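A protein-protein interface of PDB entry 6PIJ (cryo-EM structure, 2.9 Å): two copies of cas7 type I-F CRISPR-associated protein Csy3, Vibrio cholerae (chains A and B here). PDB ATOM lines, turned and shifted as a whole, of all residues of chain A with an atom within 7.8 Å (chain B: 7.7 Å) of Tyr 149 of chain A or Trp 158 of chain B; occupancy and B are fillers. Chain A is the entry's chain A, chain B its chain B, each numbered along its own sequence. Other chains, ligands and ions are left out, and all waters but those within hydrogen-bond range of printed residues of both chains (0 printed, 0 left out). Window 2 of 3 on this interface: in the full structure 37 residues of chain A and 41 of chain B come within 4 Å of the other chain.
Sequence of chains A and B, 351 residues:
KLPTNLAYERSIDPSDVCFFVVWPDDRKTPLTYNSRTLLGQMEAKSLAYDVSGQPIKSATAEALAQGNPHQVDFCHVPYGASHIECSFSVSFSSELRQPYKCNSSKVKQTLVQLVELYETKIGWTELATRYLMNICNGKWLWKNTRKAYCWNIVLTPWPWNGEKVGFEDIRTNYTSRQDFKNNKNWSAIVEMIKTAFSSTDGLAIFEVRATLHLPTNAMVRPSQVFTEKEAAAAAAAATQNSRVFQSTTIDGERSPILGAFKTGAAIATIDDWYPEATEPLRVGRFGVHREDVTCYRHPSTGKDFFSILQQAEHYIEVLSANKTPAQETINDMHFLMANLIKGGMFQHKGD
Of the 18 printed residues of chain B, 6 touch a printed residue of chain A.
Printed residues of chain B that touch a printed residue of chain A: Ser 89, Ser 91, Trp 158, Leu 203, Ile 205 and Glu 207.
Hydrophobic or aromatic side chains of chain B within 4 Å of the printed part of chain A: Trp 158, Leu 203 and Ile 205.
Along chain B the printed residues that touch a printed residue of chain A span positions 89 to 207.
Hydrophobic or aromatic side chains of chain A that line the printed part of chain B: Tyr 149 and Pro 215.
Among the printed residues, 11 pairs touch across the chains.
Among the printed residues, no Asp or Glu carboxylate lies within 4 Å of a Lys or Arg side-chain nitrogen of the other chain.
The backbone carbonyl oxygen of Tyr 149 of chain A lies within hydrogen-bond range of the guanidinium group of Arg 171 of chain A (3.5 Å).
N of Tyr 149 of chain A is in hydrogen-bond range of O of His 213 of chain A (2.9 Å).
The backbone NH (N) of Thr 156 of chain B sits at hydrogen-bond distance from the backbone carbonyl oxygen (O) of Glu 207 of chain B (3.0 Å).
The backbone NH (N) of Trp 158 of chain B is in hydrogen-bond range of the backbone carbonyl oxygen (O) of Ile 205 of chain B.
Tyr 149 of chain A touches just these residues of chain B: Trp 158 (3.5 Å), Ile 205 (3.5 Å) and Glu 207 (3.4 Å).
Of chain A, only Tyr 149 (3.5 Å) comes within 4 Å of Trp 158 of chain B.
No residue of chain B comes within 4 Å of Ala 148 of chain A.
No residue of chain A comes within 4 Å of Pro 159 of chain B.
Printed residues of chain A within 4 Å of Ile 205 of chain B: Lys 147, Tyr 149 and Pro 215.
Of the printed residues of chain A, Leu 203 of chain B touches Lys 147.
The nearest residue of chain A that does not touch Trp 158 of chain B is Arg 171 of chain A (4.1 Å).
The nearest printed residue of chain A that does not touch Ser 91 of chain B is Pro 215 of chain A (4.4 Å).
Lys 147 of chain A touches Ser 91 of chain B.
Leu 203 of chain B touches Lys 147 of chain A (CD2 to CA, 3.8 Å).
Lys 147 of chain A touches Ile 205 of chain B (O to CD1, 3.4 Å).
Trp 158 of chain B touches Tyr 149 of chain A.
Tyr 149 of chain A touches Ile 205 of chain B.
Glu 207 of chain B touches Tyr 149 of chain A (CD to OH, 3.4 Å).
Ser 89 of chain B touches Pro 215 of chain A.
Glu 207 of chain B touches Pro 215 of chain A.
No position is printed for both chains.
Of the 11 pairs that touch across the chains among the printed residues, none has its exchanged pair printed and touching as well.
The side-chain hydroxyl (OG) of Ser 89 of chain B sits at hydrogen-bond distance from the backbone carbonyl oxygen (O) of Thr 216 of chain A, 2.7 Å away.
N of Thr 216 of chain A lies within hydrogen-bond range of OE2 of Glu 207 of chain B (2.8 Å).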
ATOM      1  N   ASN A 144     -26.328 -24.582  -3.546  1.00  0.00           N
ATOM      2  CA  ASN A 144     -26.486 -23.404  -2.652  1.00  0.00           C
ATOM      3  C   ASN A 144     -25.334 -23.360  -1.636  1.00  0.00           C
ATOM      4  O   ASN A 144     -25.067 -22.264  -1.109  1.00  0.00           O
ATOM      5  CB  ASN A 144     -27.857 -23.402  -1.973  1.00  0.00           C
ATOM      6  CG  ASN A 144     -29.002 -23.379  -2.963  1.00  0.00           C
ATOM      7  OD1 ASN A 144     -29.130 -22.441  -3.748  1.00  0.00           O
ATOM      8  ND2 ASN A 144     -29.838 -24.404  -2.936  1.00  0.00           N
ATOM      9  N   THR A 145     -24.680 -24.501  -1.380  1.00  0.00           N
ATOM     10  CA  THR A 145     -23.492 -24.628  -0.490  1.00  0.00           C
ATOM     11  C   THR A 145     -22.271 -23.991  -1.161  1.00  0.00           C
ATOM     12  O   THR A 145     -21.455 -23.387  -0.438  1.00  0.00           O
ATOM     13  CB  THR A 145     -23.201 -26.093  -0.135  1.00  0.00           C
ATOM     14  OG1 THR A 145     -22.764 -26.773  -1.313  1.00  0.00           O
ATOM     15  CG2 THR A 145     -24.397 -26.814   0.445  1.00  0.00           C
ATOM     16  N   ARG A 146     -22.143 -24.144  -2.485  1.00  0.00           N
ATOM     17  CA  ARG A 146     -21.042 -23.554  -3.293  1.00  0.00           C
ATOM     18  C   ARG A 146     -21.175 -22.026  -3.261  1.00  0.00           C
ATOM     19  O   ARG A 146     -22.306 -21.533  -3.450  1.00  0.00           O
ATOM     20  CB  ARG A 146     -21.073 -24.084  -4.731  1.00  0.00           C
ATOM     21  CG  ARG A 146     -19.755 -23.938  -5.477  1.00  0.00           C
ATOM     22  CD  ARG A 146     -18.733 -24.981  -5.060  1.00  0.00           C
ATOM     23  NE  ARG A 146     -17.382 -24.610  -5.463  1.00  0.00           N
ATOM     24  CZ  ARG A 146     -16.878 -24.723  -6.695  1.00  0.00           C
ATOM     25  NH1 ARG A 146     -17.604 -25.205  -7.692  1.00  0.00           N
ATOM     26  NH2 ARG A 146     -15.631 -24.344  -6.925  1.00  0.00           N
ATOM     27  N   LYS A 147     -20.065 -21.323  -3.001  1.00  0.00           N
ATOM     28  CA  LYS A 147     -19.976 -19.839  -2.893  1.00  0.00           C
ATOM     29  C   LYS A 147     -20.746 -19.343  -1.657  1.00  0.00           C
ATOM     30  O   LYS A 147     -21.153 -18.161  -1.658  1.00  0.00           O
ATOM     31  CB  LYS A 147     -20.499 -19.163  -4.168  1.00  0.00           C
ATOM     32  CG  LYS A 147     -19.943 -19.701  -5.480  1.00  0.00           C
ATOM     33  CD  LYS A 147     -20.847 -19.433  -6.663  1.00  0.00           C
ATOM     34  CE  LYS A 147     -20.221 -19.813  -7.989  1.00  0.00           C
ATOM     35  NZ  LYS A 147     -19.105 -18.909  -8.355  1.00  0.00           N
ATOM     36  N   ALA A 148     -20.925 -20.199  -0.642  1.00  0.00           N
ATOM     37  CA  ALA A 148     -21.476 -19.854   0.691  1.00  0.00           C
ATOM     38  C   ALA A 148     -20.314 -19.778   1.687  1.00  0.00           C
ATOM     39  O   ALA A 148     -19.297 -20.458   1.454  1.00  0.00           O
ATOM     40  CB  ALA A 148     -22.505 -20.873   1.116  1.00  0.00           C
ATOM     41  N   TYR A 149     -20.452 -18.976   2.747  1.00  0.00           N
ATOM     42  CA  TYR A 149     -19.423 -18.820   3.810  1.00  0.00           C
ATOM     43  C   TYR A 149     -19.433 -20.056   4.713  1.00  0.00           C
ATOM     44  O   TYR A 149     -18.370 -20.681   4.897  1.00  0.00           O
ATOM     45  CB  TYR A 149     -19.661 -17.555   4.640  1.00  0.00           C
ATOM     46  CG  TYR A 149     -19.361 -16.257   3.933  1.00  0.00           C
ATOM     47  CD1 TYR A 149     -18.143 -16.050   3.302  1.00  0.00           C
ATOM     48  CD2 TYR A 149     -20.281 -15.221   3.916  1.00  0.00           C
ATOM     49  CE1 TYR A 149     -17.856 -14.858   2.657  1.00  0.00           C
ATOM     50  CE2 TYR A 149     -20.008 -14.020   3.277  1.00  0.00           C
ATOM     51  CZ  TYR A 149     -18.790 -13.838   2.644  1.00  0.00           C
ATOM     52  OH  TYR A 149     -18.513 -12.660   2.013  1.00  0.00           O
ATOM     53  N   CYS A 150     -20.610 -20.385   5.252  1.00  0.00           N
ATOM     54  CA  CYS A 150     -20.824 -21.429   6.287  1.00  0.00           C
ATOM     55  C   CYS A 150     -22.254 -21.971   6.193  1.00  0.00           C
ATOM     56  O   CYS A 150     -23.167 -21.177   5.867  1.00  0.00           O
ATOM     57  CB  CYS A 150     -20.580 -20.850   7.676  1.00  0.00           C
ATOM     58  SG  CYS A 150     -20.930 -22.009   9.026  1.00  0.00           S
ATOM     59  N   TRP A 151     -22.438 -23.267   6.468  1.00  0.00           N
ATOM     60  CA  TRP A 151     -23.779 -23.883   6.653  1.00  0.00           C
ATOM     61  C   TRP A 151     -23.739 -24.953   7.750  1.00  0.00           C
ATOM     62  O   TRP A 151     -22.746 -25.707   7.817  1.00  0.00           O
ATOM     63  CB  TRP A 151     -24.344 -24.409   5.326  1.00  0.00           C
ATOM     64  CG  TRP A 151     -23.719 -25.654   4.774  1.00  0.00           C
ATOM     65  CD1 TRP A 151     -24.178 -26.932   4.903  1.00  0.00           C
ATOM     66  CD2 TRP A 151     -22.545 -25.732   3.946  1.00  0.00           C
ATOM     67  NE1 TRP A 151     -23.361 -27.801   4.233  1.00  0.00           N
ATOM     68  CE2 TRP A 151     -22.349 -27.096   3.637  1.00  0.00           C
ATOM     69  CE3 TRP A 151     -21.636 -24.790   3.449  1.00  0.00           C
ATOM     70  CZ2 TRP A 151     -21.281 -27.535   2.854  1.00  0.00           C
ATOM     71  CZ3 TRP A 151     -20.581 -25.223   2.674  1.00  0.00           C
ATOM     72  CH2 TRP A 151     -20.407 -26.579   2.384  1.00  0.00           C
ATOM     73  N   ASP A 169     -20.028 -25.828  10.961  1.00  0.00           N
ATOM     74  CA  ASP A 169     -19.345 -25.463   9.684  1.00  0.00           C
ATOM     75  C   ASP A 169     -18.765 -26.714   9.007  1.00  0.00           C
ATOM     76  O   ASP A 169     -17.717 -27.208   9.464  1.00  0.00           O
ATOM     77  CB  ASP A 169     -18.261 -24.405   9.928  1.00  0.00           C
ATOM     78  CG  ASP A 169     -17.592 -23.875   8.668  1.00  0.00           C
ATOM     79  OD1 ASP A 169     -18.241 -23.880   7.600  1.00  0.00           O
ATOM     80  OD2 ASP A 169     -16.422 -23.452   8.766  1.00  0.00           O
ATOM     81  N   ILE A 170     -19.422 -27.180   7.939  1.00  0.00           N
ATOM     82  CA  ILE A 170     -19.207 -28.518   7.307  1.00  0.00           C
ATOM     83  C   ILE A 170     -18.029 -28.451   6.325  1.00  0.00           C
ATOM     84  O   ILE A 170     -17.302 -29.460   6.232  1.00  0.00           O
ATOM     85  CB  ILE A 170     -20.517 -29.014   6.657  1.00  0.00           C
ATOM     86  CG1 ILE A 170     -21.606 -29.124   7.729  1.00  0.00           C
ATOM     87  CG2 ILE A 170     -20.315 -30.319   5.891  1.00  0.00           C
ATOM     88  CD1 ILE A 170     -22.919 -29.680   7.265  1.00  0.00           C
ATOM     89  N   ARG A 171     -17.840 -27.318   5.636  1.00  0.00           N
ATOM     90  CA  ARG A 171     -16.704 -27.083   4.698  1.00  0.00           C
ATOM     91  C   ARG A 171     -15.377 -27.483   5.364  1.00  0.00           C
ATOM     92  O   ARG A 171     -14.531 -28.076   4.662  1.00  0.00           O
ATOM     93  CB  ARG A 171     -16.670 -25.620   4.237  1.00  0.00           C
ATOM     94  CG  ARG A 171     -15.397 -25.225   3.498  1.00  0.00           C
ATOM     95  CD  ARG A 171     -15.528 -23.975   2.651  1.00  0.00           C
ATOM     96  NE  ARG A 171     -16.390 -24.188   1.489  1.00  0.00           N
ATOM     97  CZ  ARG A 171     -17.505 -23.513   1.192  1.00  0.00           C
ATOM     98  NH1 ARG A 171     -17.945 -22.529   1.963  1.00  0.00           N
ATOM     99  NH2 ARG A 171     -18.184 -23.828   0.100  1.00  0.00           N
ATOM    100  N   THR A 172     -15.208 -27.181   6.659  1.00  0.00           N
ATOM    101  CA  THR A 172     -13.937 -27.332   7.423  1.00  0.00           C
ATOM    102  C   THR A 172     -14.006 -28.532   8.378  1.00  0.00           C
ATOM    103  O   THR A 172     -13.119 -29.404   8.277  1.00  0.00           O
ATOM    104  CB  THR A 172     -13.608 -26.037   8.178  1.00  0.00           C
ATOM    105  OG1 THR A 172     -14.514 -25.890   9.273  1.00  0.00           O
ATOM    106  CG2 THR A 172     -13.691 -24.809   7.296  1.00  0.00           C
ATOM    107  N   LEU A 212     -27.790 -21.548   6.385  1.00  0.00           N
ATOM    108  CA  LEU A 212     -26.894 -21.304   5.217  1.00  0.00           C
ATOM    109  C   LEU A 212     -26.568 -19.807   5.123  1.00  0.00           C
ATOM    110  O   LEU A 212     -27.477 -19.029   4.772  1.00  0.00           O
ATOM    111  CB  LEU A 212     -27.596 -21.821   3.955  1.00  0.00           C
ATOM    112  CG  LEU A 212     -26.834 -21.699   2.634  1.00  0.00           C
ATOM    113  CD1 LEU A 212     -25.467 -22.360   2.699  1.00  0.00           C
ATOM    114  CD2 LEU A 212     -27.641 -22.310   1.499  1.00  0.00           C
ATOM    115  N   HIS A 213     -25.318 -19.432   5.429  1.00  0.00           N
ATOM    116  CA  HIS A 213     -24.808 -18.032   5.420  1.00  0.00           C
ATOM    117  C   HIS A 213     -24.168 -17.726   4.061  1.00  0.00           C
ATOM    118  O   HIS A 213     -23.027 -18.185   3.822  1.00  0.00           O
ATOM    119  CB  HIS A 213     -23.820 -17.801   6.572  1.00  0.00           C
ATOM    120  CG  HIS A 213     -24.426 -17.899   7.932  1.00  0.00           C
ATOM    121  ND1 HIS A 213     -24.315 -16.885   8.864  1.00  0.00           N
ATOM    122  CD2 HIS A 213     -25.139 -18.882   8.525  1.00  0.00           C
ATOM    123  CE1 HIS A 213     -24.934 -17.240   9.972  1.00  0.00           C
ATOM    124  NE2 HIS A 213     -25.449 -18.461   9.789  1.00  0.00           N
ATOM    125  N   LEU A 214     -24.882 -16.977   3.213  1.00  0.00           N
ATOM    126  CA  LEU A 214     -24.446 -16.569   1.850  1.00  0.00           C
ATOM    127  C   LEU A 214     -23.944 -15.125   1.897  1.00  0.00           C
ATOM    128  O   LEU A 214     -24.298 -14.382   2.811  1.00  0.00           O
ATOM    129  CB  LEU A 214     -25.629 -16.715   0.887  1.00  0.00           C
ATOM    130  CG  LEU A 214     -26.232 -18.116   0.779  1.00  0.00           C
ATOM    131  CD1 LEU A 214     -27.636 -18.065   0.199  1.00  0.00           C
ATOM    132  CD2 LEU A 214     -25.346 -19.023  -0.058  1.00  0.00           C
ATOM    133  N   PRO A 215     -23.099 -14.682   0.933  1.00  0.00           N
ATOM    134  CA  PRO A 215     -22.692 -13.276   0.847  1.00  0.00           C
ATOM    135  C   PRO A 215     -23.846 -12.317   0.499  1.00  0.00           C
ATOM    136  O   PRO A 215     -24.968 -12.768   0.346  1.00  0.00           O
ATOM    137  CB  PRO A 215     -21.598 -13.263  -0.237  1.00  0.00           C
ATOM    138  CG  PRO A 215     -21.824 -14.525  -1.043  1.00  0.00           C
ATOM    139  CD  PRO A 215     -22.442 -15.520  -0.084  1.00  0.00           C
ATOM    140  N   THR A 216     -23.545 -11.015   0.410  1.00  0.00           N
ATOM    141  CA  THR A 216     -24.527  -9.911   0.207  1.00  0.00           C
ATOM    142  C   THR A 216     -25.218 -10.068  -1.155  1.00  0.00           C
ATOM    143  O   THR A 216     -24.499 -10.192  -2.165  1.00  0.00           O
ATOM    144  CB  THR A 216     -23.853  -8.537   0.328  1.00  0.00           C
ATOM    145  OG1 THR A 216     -23.430  -8.380   1.682  1.00  0.00           O
ATOM    146  CG2 THR A 216     -24.758  -7.386  -0.060  1.00  0.00           C
ATOM    147  N   ALA A 218     -26.658 -12.504  -2.452  1.00  0.00           N
ATOM    148  CA  ALA A 218     -26.215 -13.779  -3.066  1.00  0.00           C
ATOM    149  C   ALA A 218     -27.413 -14.476  -3.719  1.00  0.00           C
ATOM    150  O   ALA A 218     -28.530 -14.382  -3.173  1.00  0.00           O
ATOM    151  CB  ALA A 218     -25.559 -14.667  -2.041  1.00  0.00           C
ATOM    152  N   SER B  89     -21.591  -8.107  -3.851  1.00  0.00           N
ATOM    153  CA  SER B  89     -20.643  -9.228  -3.605  1.00  0.00           C
ATOM    154  C   SER B  89     -20.279  -9.922  -4.925  1.00  0.00           C
ATOM    155  O   SER B  89     -21.173 -10.062  -5.781  1.00  0.00           O
ATOM    156  CB  SER B  89     -21.221 -10.209  -2.616  1.00  0.00           C
ATOM    157  OG  SER B  89     -22.200 -11.037  -3.227  1.00  0.00           O
ATOM    158  N   VAL B  90     -19.015 -10.341  -5.064  1.00  0.00           N
ATOM    159  CA  VAL B  90     -18.488 -11.162  -6.198  1.00  0.00           C
ATOM    160  C   VAL B  90     -17.929 -12.472  -5.630  1.00  0.00           C
ATOM    161  O   VAL B  90     -17.392 -12.448  -4.500  1.00  0.00           O
ATOM    162  CB  VAL B  90     -17.406 -10.421  -7.008  1.00  0.00           C
ATOM    163  CG1 VAL B  90     -17.263 -11.008  -8.405  1.00  0.00           C
ATOM    164  CG2 VAL B  90     -17.666  -8.925  -7.085  1.00  0.00           C
ATOM    165  N   SER B  91     -18.039 -13.559  -6.402  1.00  0.00           N
ATOM    166  CA  SER B  91     -17.514 -14.912  -6.080  1.00  0.00           C
ATOM    167  C   SER B  91     -16.707 -15.444  -7.271  1.00  0.00           C
ATOM    168  O   SER B  91     -17.294 -15.556  -8.370  1.00  0.00           O
ATOM    169  CB  SER B  91     -18.634 -15.856  -5.722  1.00  0.00           C
ATOM    170  OG  SER B  91     -19.445 -15.317  -4.688  1.00  0.00           O
ATOM    171  N   PHE B  92     -15.419 -15.742  -7.053  1.00  0.00           N
ATOM    172  CA  PHE B  92     -14.494 -16.361  -8.041  1.00  0.00           C
ATOM    173  C   PHE B  92     -14.333 -17.849  -7.708  1.00  0.00           C
ATOM    174  O   PHE B  92     -13.879 -18.158  -6.584  1.00  0.00           O
ATOM    175  CB  PHE B  92     -13.141 -15.646  -8.046  1.00  0.00           C
ATOM    176  CG  PHE B  92     -13.197 -14.222  -8.533  1.00  0.00           C
ATOM    177  CD1 PHE B  92     -13.563 -13.195  -7.674  1.00  0.00           C
ATOM    178  CD2 PHE B  92     -12.902 -13.907  -9.852  1.00  0.00           C
ATOM    179  CE1 PHE B  92     -13.623 -11.884  -8.121  1.00  0.00           C
ATOM    180  CE2 PHE B  92     -12.962 -12.595 -10.298  1.00  0.00           C
ATOM    181  CZ  PHE B  92     -13.322 -11.586  -9.432  1.00  0.00           C
ATOM    182  N   LEU B 155     -12.877  -3.203  -0.240  1.00  0.00           N
ATOM    183  CA  LEU B 155     -13.038  -4.676  -0.389  1.00  0.00           C
ATOM    184  C   LEU B 155     -12.893  -5.338   0.987  1.00  0.00           C
ATOM    185  O   LEU B 155     -11.895  -5.022   1.689  1.00  0.00           O
ATOM    186  CB  LEU B 155     -11.976  -5.222  -1.352  1.00  0.00           C
ATOM    187  CG  LEU B 155     -12.287  -5.113  -2.844  1.00  0.00           C
ATOM    188  CD1 LEU B 155     -12.234  -3.668  -3.316  1.00  0.00           C
ATOM    189  CD2 LEU B 155     -11.321  -5.968  -3.654  1.00  0.00           C
ATOM    190  N   THR B 156     -13.840  -6.216   1.344  1.00  0.00           N
ATOM    191  CA  THR B 156     -13.710  -7.214   2.445  1.00  0.00           C
ATOM    192  C   THR B 156     -13.701  -8.606   1.811  1.00  0.00           C
ATOM    193  O   THR B 156     -14.756  -9.185   1.552  1.00  0.00           O
ATOM    194  CB  THR B 156     -14.752  -7.008   3.557  1.00  0.00           C
ATOM    195  OG1 THR B 156     -14.638  -8.102   4.468  1.00  0.00           O
ATOM    196  CG2 THR B 156     -16.185  -6.904   3.081  1.00  0.00           C
ATOM    197  N   PRO B 157     -12.504  -9.164   1.502  1.00  0.00           N
ATOM    198  CA  PRO B 157     -12.396 -10.480   0.870  1.00  0.00           C
ATOM    199  C   PRO B 157     -12.537 -11.656   1.849  1.00  0.00           C
ATOM    200  O   PRO B 157     -12.640 -11.430   3.042  1.00  0.00           O
ATOM    201  CB  PRO B 157     -10.995 -10.454   0.240  1.00  0.00           C
ATOM    202  CG  PRO B 157     -10.195  -9.508   1.104  1.00  0.00           C
ATOM    203  CD  PRO B 157     -11.188  -8.545   1.719  1.00  0.00           C
ATOM    204  N   TRP B 158     -12.541 -12.878   1.305  1.00  0.00           N
ATOM    205  CA  TRP B 158     -12.720 -14.156   2.046  1.00  0.00           C
ATOM    206  C   TRP B 158     -12.246 -15.320   1.172  1.00  0.00           C
ATOM    207  O   TRP B 158     -12.584 -15.360  -0.011  1.00  0.00           O
ATOM    208  CB  TRP B 158     -14.189 -14.319   2.462  1.00  0.00           C
ATOM    209  CG  TRP B 158     -14.458 -15.530   3.302  1.00  0.00           C
ATOM    210  CD1 TRP B 158     -14.535 -15.586   4.663  1.00  0.00           C
ATOM    211  CD2 TRP B 158     -14.685 -16.871   2.832  1.00  0.00           C
ATOM    212  NE1 TRP B 158     -14.795 -16.866   5.073  1.00  0.00           N
ATOM    213  CE2 TRP B 158     -14.890 -17.677   3.973  1.00  0.00           C
ATOM    214  CE3 TRP B 158     -14.736 -17.468   1.566  1.00  0.00           C
ATOM    215  CZ2 TRP B 158     -15.144 -19.047   3.879  1.00  0.00           C
ATOM    216  CZ3 TRP B 158     -14.982 -18.821   1.473  1.00  0.00           C
ATOM    217  CH2 TRP B 158     -15.184 -19.598   2.617  1.00  0.00           C
ATOM    218  N   PRO B 159     -11.466 -16.306   1.687  1.00  0.00           N
ATOM    219  CA  PRO B 159     -10.973 -16.325   3.069  1.00  0.00           C
ATOM    220  C   PRO B 159      -9.829 -15.321   3.283  1.00  0.00           C
ATOM    221  O   PRO B 159      -8.990 -15.200   2.407  1.00  0.00           O
ATOM    222  CB  PRO B 159     -10.475 -17.766   3.243  1.00  0.00           C
ATOM    223  CG  PRO B 159     -10.010 -18.151   1.858  1.00  0.00           C
ATOM    224  CD  PRO B 159     -11.000 -17.479   0.930  1.00  0.00           C
ATOM    225  N   TRP B 160      -9.825 -14.646   4.437  1.00  0.00           N
ATOM    226  CA  TRP B 160      -8.971 -13.458   4.717  1.00  0.00           C
ATOM    227  C   TRP B 160      -8.578 -13.400   6.197  1.00  0.00           C
ATOM    228  O   TRP B 160      -9.381 -13.840   7.046  1.00  0.00           O
ATOM    229  CB  TRP B 160      -9.715 -12.187   4.297  1.00  0.00           C
ATOM    230  CG  TRP B 160      -8.865 -10.960   4.174  1.00  0.00           C
ATOM    231  CD1 TRP B 160      -8.994  -9.798   4.878  1.00  0.00           C
ATOM    232  CD2 TRP B 160      -7.774 -10.754   3.258  1.00  0.00           C
ATOM    233  NE1 TRP B 160      -8.059  -8.887   4.469  1.00  0.00           N
ATOM    234  CE2 TRP B 160      -7.298  -9.442   3.475  1.00  0.00           C
ATOM    235  CE3 TRP B 160      -7.162 -11.539   2.273  1.00  0.00           C
ATOM    236  CZ2 TRP B 160      -6.230  -8.909   2.751  1.00  0.00           C
ATOM    237  CZ3 TRP B 160      -6.107 -11.013   1.559  1.00  0.00           C
ATOM    238  CH2 TRP B 160      -5.649  -9.714   1.797  1.00  0.00           C
ATOM    239  N   ASN B 161      -7.381 -12.872   6.473  1.00  0.00           N
ATOM    240  CA  ASN B 161      -6.944 -12.412   7.818  1.00  0.00           C
ATOM    241  C   ASN B 161      -6.171 -11.095   7.667  1.00  0.00           C
ATOM    242  O   ASN B 161      -5.258 -11.035   6.817  1.00  0.00           O
ATOM    243  CB  ASN B 161      -6.129 -13.472   8.571  1.00  0.00           C
ATOM    244  CG  ASN B 161      -4.957 -14.035   7.789  1.00  0.00           C
ATOM    245  OD1 ASN B 161      -3.939 -13.369   7.612  1.00  0.00           O
ATOM    246  ND2 ASN B 161      -5.076 -15.277   7.348  1.00  0.00           N
ATOM    247  N   ILE B 189      -4.358 -10.244  -2.935  1.00  0.00           N
ATOM    248  CA  ILE B 189      -5.767 -10.424  -3.416  1.00  0.00           C
ATOM    249  C   ILE B 189      -5.791 -10.817  -4.903  1.00  0.00           C
ATOM    250  O   ILE B 189      -6.796 -11.432  -5.305  1.00  0.00           O
ATOM    251  CB  ILE B 189      -6.653  -9.192  -3.126  1.00  0.00           C
ATOM    252  CG1 ILE B 189      -6.140  -7.908  -3.787  1.00  0.00           C
ATOM    253  CG2 ILE B 189      -6.842  -9.017  -1.625  1.00  0.00           C
ATOM    254  CD1 ILE B 189      -7.069  -6.723  -3.647  1.00  0.00           C
ATOM    255  N   MET B 192      -4.980 -15.734  -4.587  1.00  0.00           N
ATOM    256  CA  MET B 192      -6.275 -16.193  -3.999  1.00  0.00           C
ATOM    257  C   MET B 192      -7.362 -16.186  -5.088  1.00  0.00           C
ATOM    258  O   MET B 192      -8.294 -16.998  -4.958  1.00  0.00           O
ATOM    259  CB  MET B 192      -6.726 -15.416  -2.749  1.00  0.00           C
ATOM    260  CG  MET B 192      -7.696 -14.260  -2.991  1.00  0.00           C
ATOM    261  SD  MET B 192      -8.088 -13.372  -1.460  1.00  0.00           S
ATOM    262  CE  MET B 192      -9.382 -14.420  -0.794  1.00  0.00           C
ATOM    263  N   LEU B 203     -12.315 -21.319  -4.124  1.00  0.00           N
ATOM    264  CA  LEU B 203     -13.332 -20.246  -3.960  1.00  0.00           C
ATOM    265  C   LEU B 203     -12.667 -18.996  -3.372  1.00  0.00           C
ATOM    266  O   LEU B 203     -11.904 -19.141  -2.393  1.00  0.00           O
ATOM    267  CB  LEU B 203     -14.445 -20.777  -3.047  1.00  0.00           C
ATOM    268  CG  LEU B 203     -15.470 -19.757  -2.549  1.00  0.00           C
ATOM    269  CD1 LEU B 203     -16.182 -19.072  -3.707  1.00  0.00           C
ATOM    270  CD2 LEU B 203     -16.480 -20.425  -1.629  1.00  0.00           C
ATOM    271  N   ALA B 204     -12.945 -17.826  -3.956  1.00  0.00           N
ATOM    272  CA  ALA B 204     -12.579 -16.495  -3.414  1.00  0.00           C
ATOM    273  C   ALA B 204     -13.788 -15.559  -3.507  1.00  0.00           C
ATOM    274  O   ALA B 204     -14.130 -15.146  -4.636  1.00  0.00           O
ATOM    275  CB  ALA B 204     -11.390 -15.941  -4.157  1.00  0.00           C
ATOM    276  N   ILE B 205     -14.417 -15.260  -2.365  1.00  0.00           N
ATOM    277  CA  ILE B 205     -15.552 -14.294  -2.253  1.00  0.00           C
ATOM    278  C   ILE B 205     -14.974 -12.921  -1.891  1.00  0.00           C
ATOM    279  O   ILE B 205     -14.066 -12.867  -1.040  1.00  0.00           O
ATOM    280  CB  ILE B 205     -16.606 -14.768  -1.228  1.00  0.00           C
ATOM    281  CG1 ILE B 205     -17.059 -16.203  -1.518  1.00  0.00           C
ATOM    282  CG2 ILE B 205     -17.782 -13.795  -1.171  1.00  0.00           C
ATOM    283  CD1 ILE B 205     -18.240 -16.677  -0.697  1.00  0.00           C
ATOM    284  N   PHE B 206     -15.482 -11.866  -2.533  1.00  0.00           N
ATOM    285  CA  PHE B 206     -15.224 -10.443  -2.191  1.00  0.00           C
ATOM    286  C   PHE B 206     -16.571  -9.751  -1.966  1.00  0.00           C
ATOM    287  O   PHE B 206     -17.507 -10.034  -2.733  1.00  0.00           O
ATOM    288  CB  PHE B 206     -14.427  -9.753  -3.302  1.00  0.00           C
ATOM    289  CG  PHE B 206     -13.073 -10.357  -3.583  1.00  0.00           C
ATOM    290  CD1 PHE B 206     -12.951 -11.510  -4.344  1.00  0.00           C
ATOM    291  CD2 PHE B 206     -11.916  -9.766  -3.095  1.00  0.00           C
ATOM    292  CE1 PHE B 206     -11.704 -12.063  -4.602  1.00  0.00           C
ATOM    293  CE2 PHE B 206     -10.670 -10.320  -3.353  1.00  0.00           C
ATOM    294  CZ  PHE B 206     -10.566 -11.469  -4.105  1.00  0.00           C
ATOM    295  N   GLU B 207     -16.672  -8.905  -0.936  1.00  0.00           N
ATOM    296  CA  GLU B 207     -17.837  -8.005  -0.711  1.00  0.00           C
ATOM    297  C   GLU B 207     -17.355  -6.561  -0.878  1.00  0.00           C
ATOM    298  O   GLU B 207     -16.536  -6.108  -0.051  1.00  0.00           O
ATOM    299  CB  GLU B 207     -18.486  -8.282   0.646  1.00  0.00           C
ATOM    300  CG  GLU B 207     -19.536  -9.381   0.589  1.00  0.00           C
ATOM    301  CD  GLU B 207     -20.246  -9.684   1.899  1.00  0.00           C
ATOM    302  OE1 GLU B 207     -19.796  -9.188   2.952  1.00  0.00           O
ATOM    303  OE2 GLU B 207     -21.254 -10.419   1.860  1.00  0.00           O
